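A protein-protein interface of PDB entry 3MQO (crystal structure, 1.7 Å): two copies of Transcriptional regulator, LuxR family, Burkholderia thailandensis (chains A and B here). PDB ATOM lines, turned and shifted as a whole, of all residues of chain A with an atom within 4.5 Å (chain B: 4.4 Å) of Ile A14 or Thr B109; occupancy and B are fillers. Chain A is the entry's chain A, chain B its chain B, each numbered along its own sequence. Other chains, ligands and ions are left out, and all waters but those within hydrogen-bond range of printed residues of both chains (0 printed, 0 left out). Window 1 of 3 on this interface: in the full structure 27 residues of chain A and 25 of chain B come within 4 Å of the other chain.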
ATOM      1  N   ALA A  12      14.170  27.433  -5.721  1.00  0.00           N
ATOM      2  CA  ALA A  12      12.711  27.521  -5.884  1.00  0.00           C
ATOM      3  C   ALA A  12      12.302  28.325  -7.111  1.00  0.00           C
ATOM      4  O   ALA A  12      12.893  29.344  -7.379  1.00  0.00           O
ATOM      5  CB  ALA A  12      12.054  28.107  -4.616  1.00  0.00           C
ATOM      6  N   PRO A  13      11.263  27.872  -7.842  1.00  0.00           N
ATOM      7  CA  PRO A  13      10.840  28.524  -9.096  1.00  0.00           C
ATOM      8  C   PRO A  13      10.037  29.827  -8.919  1.00  0.00           C
ATOM      9  O   PRO A  13       9.588  30.436  -9.912  1.00  0.00           O
ATOM     10  CB  PRO A  13       9.974  27.456  -9.759  1.00  0.00           C
ATOM     11  CG  PRO A  13       9.448  26.658  -8.630  1.00  0.00           C
ATOM     12  CD  PRO A  13      10.507  26.631  -7.590  1.00  0.00           C
ATOM     13  N   ILE A  14       9.809  30.196  -7.663  1.00  0.00           N
ATOM     14  CA  ILE A  14       9.140  31.442  -7.278  1.00  0.00           C
ATOM     15  C   ILE A  14      10.051  32.269  -6.373  1.00  0.00           C
ATOM     16  O   ILE A  14      10.919  31.714  -5.691  1.00  0.00           O
ATOM     17  CB  ILE A  14       7.757  31.200  -6.571  1.00  0.00           C
ATOM     18  CG1 ILE A  14       7.905  30.774  -5.099  1.00  0.00           C
ATOM     19  CG2 ILE A  14       6.882  30.234  -7.375  1.00  0.00           C
ATOM     20  CD1 ILE A  14       8.721  29.514  -4.861  1.00  0.00           C
ATOM     21  N   GLY A  15       9.846  33.581  -6.356  1.00  0.00           N
ATOM     22  CA  GLY A  15      10.582  34.450  -5.440  1.00  0.00           C
ATOM     23  C   GLY A  15      10.214  34.132  -4.003  1.00  0.00           C
ATOM     24  O   GLY A  15       9.025  34.034  -3.667  1.00  0.00           O
ATOM     25  N   LEU A  16      11.218  33.909  -3.158  1.00  0.00           N
ATOM     26  CA  LEU A  16      10.960  33.627  -1.751  1.00  0.00           C
ATOM     27  C   LEU A  16      11.679  34.627  -0.903  1.00  0.00           C
ATOM     28  O   LEU A  16      12.785  35.068  -1.263  1.00  0.00           O
ATOM     29  CB  LEU A  16      11.463  32.243  -1.344  1.00  0.00           C
ATOM     30  CG  LEU A  16      10.713  31.060  -1.927  1.00  0.00           C
ATOM     31  CD1 LEU A  16      11.409  29.771  -1.478  1.00  0.00           C
ATOM     32  CD2 LEU A  16       9.208  31.136  -1.552  1.00  0.00           C
ATOM     33  N   ASN A  28      15.815  34.572  -2.486  1.00  0.00           N
ATOM     34  CA  ASN A  28      16.448  33.718  -3.500  1.00  0.00           C
ATOM     35  C   ASN A  28      16.699  34.463  -4.805  1.00  0.00           C
ATOM     36  O   ASN A  28      16.281  35.634  -4.956  1.00  0.00           O
ATOM     37  CB  ASN A  28      15.667  32.406  -3.726  1.00  0.00           C
ATOM     38  CG  ASN A  28      14.224  32.629  -4.220  1.00  0.00           C
ATOM     39  OD1 ASN A  28      13.796  33.747  -4.540  1.00  0.00           O
ATOM     40  ND2 ASN A  28      13.461  31.545  -4.245  1.00  0.00           N
ATOM     41  N   GLU A  30      15.488  33.873  -7.698  1.00  0.00           N
ATOM     42  CA  GLU A  30      14.244  34.116  -8.451  1.00  0.00           C
ATOM     43  C   GLU A  30      13.629  35.460  -8.077  1.00  0.00           C
ATOM     44  O   GLU A  30      13.072  36.161  -8.946  1.00  0.00           O
ATOM     45  CB  GLU A  30      13.240  32.985  -8.242  1.00  0.00           C
ATOM     46  CG  GLU A  30      11.967  33.092  -9.082  1.00  0.00           C
ATOM     47  CD  GLU A  30      12.209  32.937 -10.571  1.00  0.00           C
ATOM     48  OE1 GLU A  30      13.151  32.225 -10.959  1.00  0.00           O
ATOM     49  OE2 GLU A  30      11.455  33.544 -11.354  1.00  0.00           O
ATOM     50  N   THR A 109       6.148  35.056  -0.569  1.00  0.00           N
ATOM     51  CA  THR A 109       6.385  34.585  -1.923  1.00  0.00           C
ATOM     52  C   THR A 109       5.964  35.633  -2.935  1.00  0.00           C
ATOM     53  O   THR A 109       5.016  36.383  -2.716  1.00  0.00           O
ATOM     54  CB  THR A 109       5.660  33.254  -2.225  1.00  0.00           C
ATOM     55  OG1 THR A 109       4.281  33.531  -2.498  1.00  0.00           O
ATOM     56  CG2 THR A 109       5.758  32.268  -1.075  1.00  0.00           C
ATOM     57  N   PHE A 110       6.687  35.676  -4.056  1.00  0.00           N
ATOM     58  CA  PHE A 110       6.448  36.610  -5.120  1.00  0.00           C
ATOM     59  C   PHE A 110       6.511  35.865  -6.452  1.00  0.00           C
ATOM     60  O   PHE A 110       7.425  35.089  -6.677  1.00  0.00           O
ATOM     61  CB  PHE A 110       7.539  37.681  -5.097  1.00  0.00           C
ATOM     62  CG  PHE A 110       7.511  38.540  -3.871  1.00  0.00           C
ATOM     63  CD1 PHE A 110       6.894  39.789  -3.901  1.00  0.00           C
ATOM     64  CD2 PHE A 110       8.086  38.101  -2.687  1.00  0.00           C
ATOM     65  CE1 PHE A 110       6.837  40.576  -2.764  1.00  0.00           C
ATOM     66  CE2 PHE A 110       8.031  38.888  -1.530  1.00  0.00           C
ATOM     67  CZ  PHE A 110       7.412  40.130  -1.578  1.00  0.00           C
ATOM     68  N   ILE B  14       2.395  28.555   0.792  1.00  0.00           N
ATOM     69  CA  ILE B  14       2.021  27.702  -0.343  1.00  0.00           C
ATOM     70  C   ILE B  14       2.554  26.285  -0.142  1.00  0.00           C
ATOM     71  O   ILE B  14       3.481  26.070   0.648  1.00  0.00           O
ATOM     72  CB  ILE B  14       2.533  28.260  -1.683  1.00  0.00           C
ATOM     73  CG1 ILE B  14       4.058  28.350  -1.696  1.00  0.00           C
ATOM     74  CG2 ILE B  14       1.859  29.610  -1.989  1.00  0.00           C
ATOM     75  CD1 ILE B  14       4.610  28.781  -3.003  1.00  0.00           C
ATOM     76  N   GLY B  15       1.974  25.323  -0.849  1.00  0.00           N
ATOM     77  CA  GLY B  15       2.486  23.959  -0.791  1.00  0.00           C
ATOM     78  C   GLY B  15       3.859  23.861  -1.420  1.00  0.00           C
ATOM     79  O   GLY B  15       4.076  24.347  -2.539  1.00  0.00           O
ATOM     80  N   LEU B  16       4.780  23.214  -0.706  1.00  0.00           N
ATOM     81  CA  LEU B  16       6.127  22.983  -1.212  1.00  0.00           C
ATOM     82  C   LEU B  16       6.421  21.510  -1.217  1.00  0.00           C
ATOM     83  O   LEU B  16       5.980  20.781  -0.318  1.00  0.00           O
ATOM     84  CB  LEU B  16       7.167  23.668  -0.334  1.00  0.00           C
ATOM     85  CG  LEU B  16       7.124  25.189  -0.399  1.00  0.00           C
ATOM     86  CD1 LEU B  16       8.135  25.764   0.549  1.00  0.00           C
ATOM     87  CD2 LEU B  16       7.350  25.677  -1.846  1.00  0.00           C
ATOM     88  N   HIS B  91      -2.476  25.965  -9.000  1.00  0.00           N
ATOM     89  CA  HIS B  91      -1.356  26.557  -9.719  1.00  0.00           C
ATOM     90  C   HIS B  91      -0.075  25.862  -9.253  1.00  0.00           C
ATOM     91  O   HIS B  91       0.200  25.774  -8.054  1.00  0.00           O
ATOM     92  CB  HIS B  91      -1.233  28.051  -9.444  1.00  0.00           C
ATOM     93  CG  HIS B  91      -0.156  28.709 -10.242  1.00  0.00           C
ATOM     94  ND1 HIS B  91       0.932  29.334  -9.670  1.00  0.00           N
ATOM     95  CD2 HIS B  91      -0.011  28.848 -11.582  1.00  0.00           C
ATOM     96  CE1 HIS B  91       1.702  29.826 -10.627  1.00  0.00           C
ATOM     97  NE2 HIS B  91       1.150  29.549 -11.794  1.00  0.00           N
ATOM     98  N   VAL B  92       0.694  25.354 -10.210  1.00  0.00           N
ATOM     99  CA  VAL B  92       1.897  24.569  -9.891  1.00  0.00           C
ATOM    100  C   VAL B  92       3.110  25.184 -10.585  1.00  0.00           C
ATOM    101  O   VAL B  92       3.011  25.614 -11.725  1.00  0.00           O
ATOM    102  CB  VAL B  92       1.714  23.113 -10.344  1.00  0.00           C
ATOM    103  CG1 VAL B  92       2.984  22.295 -10.137  1.00  0.00           C
ATOM    104  CG2 VAL B  92       0.571  22.487  -9.576  1.00  0.00           C
ATOM    105  N   THR B  93       4.236  25.253  -9.871  1.00  0.00           N
ATOM    106  CA  THR B  93       5.504  25.668 -10.479  1.00  0.00           C
ATOM    107  C   THR B  93       6.597  24.666 -10.105  1.00  0.00           C
ATOM    108  O   THR B  93       6.505  23.998  -9.093  1.00  0.00           O
ATOM    109  CB  THR B  93       5.930  27.113 -10.098  1.00  0.00           C
ATOM    110  OG1 THR B  93       6.528  27.150  -8.789  1.00  0.00           O
ATOM    111  CG2 THR B  93       4.742  28.073 -10.159  1.00  0.00           C
ATOM    112  N   TRP B 108       9.058  21.796  -6.181  1.00  0.00           N
ATOM    113  CA  TRP B 108       7.723  22.050  -6.728  1.00  0.00           C
ATOM    114  C   TRP B 108       6.795  22.799  -5.769  1.00  0.00           C
ATOM    115  O   TRP B 108       6.860  22.623  -4.540  1.00  0.00           O
ATOM    116  CB  TRP B 108       7.085  20.731  -7.165  1.00  0.00           C
ATOM    117  CG  TRP B 108       7.785  20.146  -8.380  1.00  0.00           C
ATOM    118  CD1 TRP B 108       8.922  19.378  -8.396  1.00  0.00           C
ATOM    119  CD2 TRP B 108       7.404  20.327  -9.744  1.00  0.00           C
ATOM    120  NE1 TRP B 108       9.266  19.071  -9.696  1.00  0.00           N
ATOM    121  CE2 TRP B 108       8.345  19.637 -10.541  1.00  0.00           C
ATOM    122  CE3 TRP B 108       6.352  21.007 -10.373  1.00  0.00           C
ATOM    123  CZ2 TRP B 108       8.257  19.597 -11.933  1.00  0.00           C
ATOM    124  CZ3 TRP B 108       6.266  20.966 -11.763  1.00  0.00           C
ATOM    125  CH2 TRP B 108       7.219  20.273 -12.522  1.00  0.00           C
ATOM    126  N   THR B 109       5.950  23.674  -6.328  1.00  0.00           N
ATOM    127  CA  THR B 109       5.026  24.439  -5.512  1.00  0.00           C
ATOM    128  C   THR B 109       3.612  24.171  -5.976  1.00  0.00           C
ATOM    129  O   THR B 109       3.387  23.878  -7.159  1.00  0.00           O
ATOM    130  CB  THR B 109       5.284  25.979  -5.557  1.00  0.00           C
ATOM    131  OG1 THR B 109       4.814  26.515  -6.797  1.00  0.00           O
ATOM    132  CG2 THR B 109       6.777  26.334  -5.364  1.00  0.00           C
ATOM    133  N   PHE B 110       2.678  24.240  -5.026  1.00  0.00           N
ATOM    134  CA  PHE B 110       1.258  24.043  -5.278  1.00  0.00           C
ATOM    135  C   PHE B 110       0.454  25.087  -4.526  1.00  0.00           C
ATOM    136  O   PHE B 110       0.688  25.310  -3.351  1.00  0.00           O
ATOM    137  CB  PHE B 110       0.808  22.657  -4.803  1.00  0.00           C
ATOM    138  CG  PHE B 110       1.544  21.531  -5.461  1.00  0.00           C
ATOM    139  CD1 PHE B 110       0.954  20.803  -6.493  1.00  0.00           C
ATOM    140  CD2 PHE B 110       2.835  21.210  -5.070  1.00  0.00           C
ATOM    141  CE1 PHE B 110       1.660  19.767  -7.127  1.00  0.00           C
ATOM    142  CE2 PHE B 110       3.539  20.177  -5.696  1.00  0.00           C
ATOM    143  CZ  PHE B 110       2.946  19.467  -6.733  1.00  0.00           C
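ND2 of Asn A28 is in hydrogen-bond range of O of Ile A14. OG1 of Thr B109 is in hydrogen-bond range of OG1 of Thr B93 (2.7 Å).
CG of Pro A13 touches OG1 of Thr B93, 3.0 Å away. Ile A14 touches Thr B93. CG2 of Thr B109 touches CD1 of Ile A14, at 3.8 Å.
Printed residues of chain B within 4 Å of Ile A14: Thr B93 (3.4 Å) and Thr B109 (3.8 Å). Of the printed residues of chain A, Thr B109 touches Ile A14. Printed residues of chain B within 4 Å of Pro A13: Thr B93. Printed residues of chain A within 4 Å of Thr B93: Pro A13 (3.0 Å) and Ile A14 (3.4 Å). Leu A16 touches none of the printed residues of chain B. The nearest printed residue of chain B that does not touch Ile A14 is Ile B14 (4.4 Å). The nearest printed residue of chain A that does not touch Thr B109 is Pro A13 (4.2 Å). The nearest printed residue of chain A that does not touch Thr B93 is Ala A12 (6.1 Å).
Of the 9 printed residues of chain B, 2 touch a printed residue of chain A. Printed residues of chain B that touch a printed residue of chain A: Thr B93 and Thr B109. Of the 9 printed residues of chain A, 2 touch a printed residue of chain B. Printed residues of chain A that touch a printed residue of chain B: Pro A13 and Ile A14. Hydrophobic or aromatic side chains of chain A that line the printed part of chain B: Pro A13 and Ile A14. Among the printed residues, 3 pairs touch across the chains. Among the printed residues, no Asp or Glu carboxylate lies within 4 Å of a Lys or Arg side-chain nitrogen of the other chain.
Ile A14 touches Thr B109, but with the chains exchanged Thr A109 does not touch Ile B14 (4.1 Å). Positions printed for both chains: 14, 15, 16, 109 and 110. Of the 3 pairs that touch across the chains among the printed residues, none has its exchanged pair printed and touching as well.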
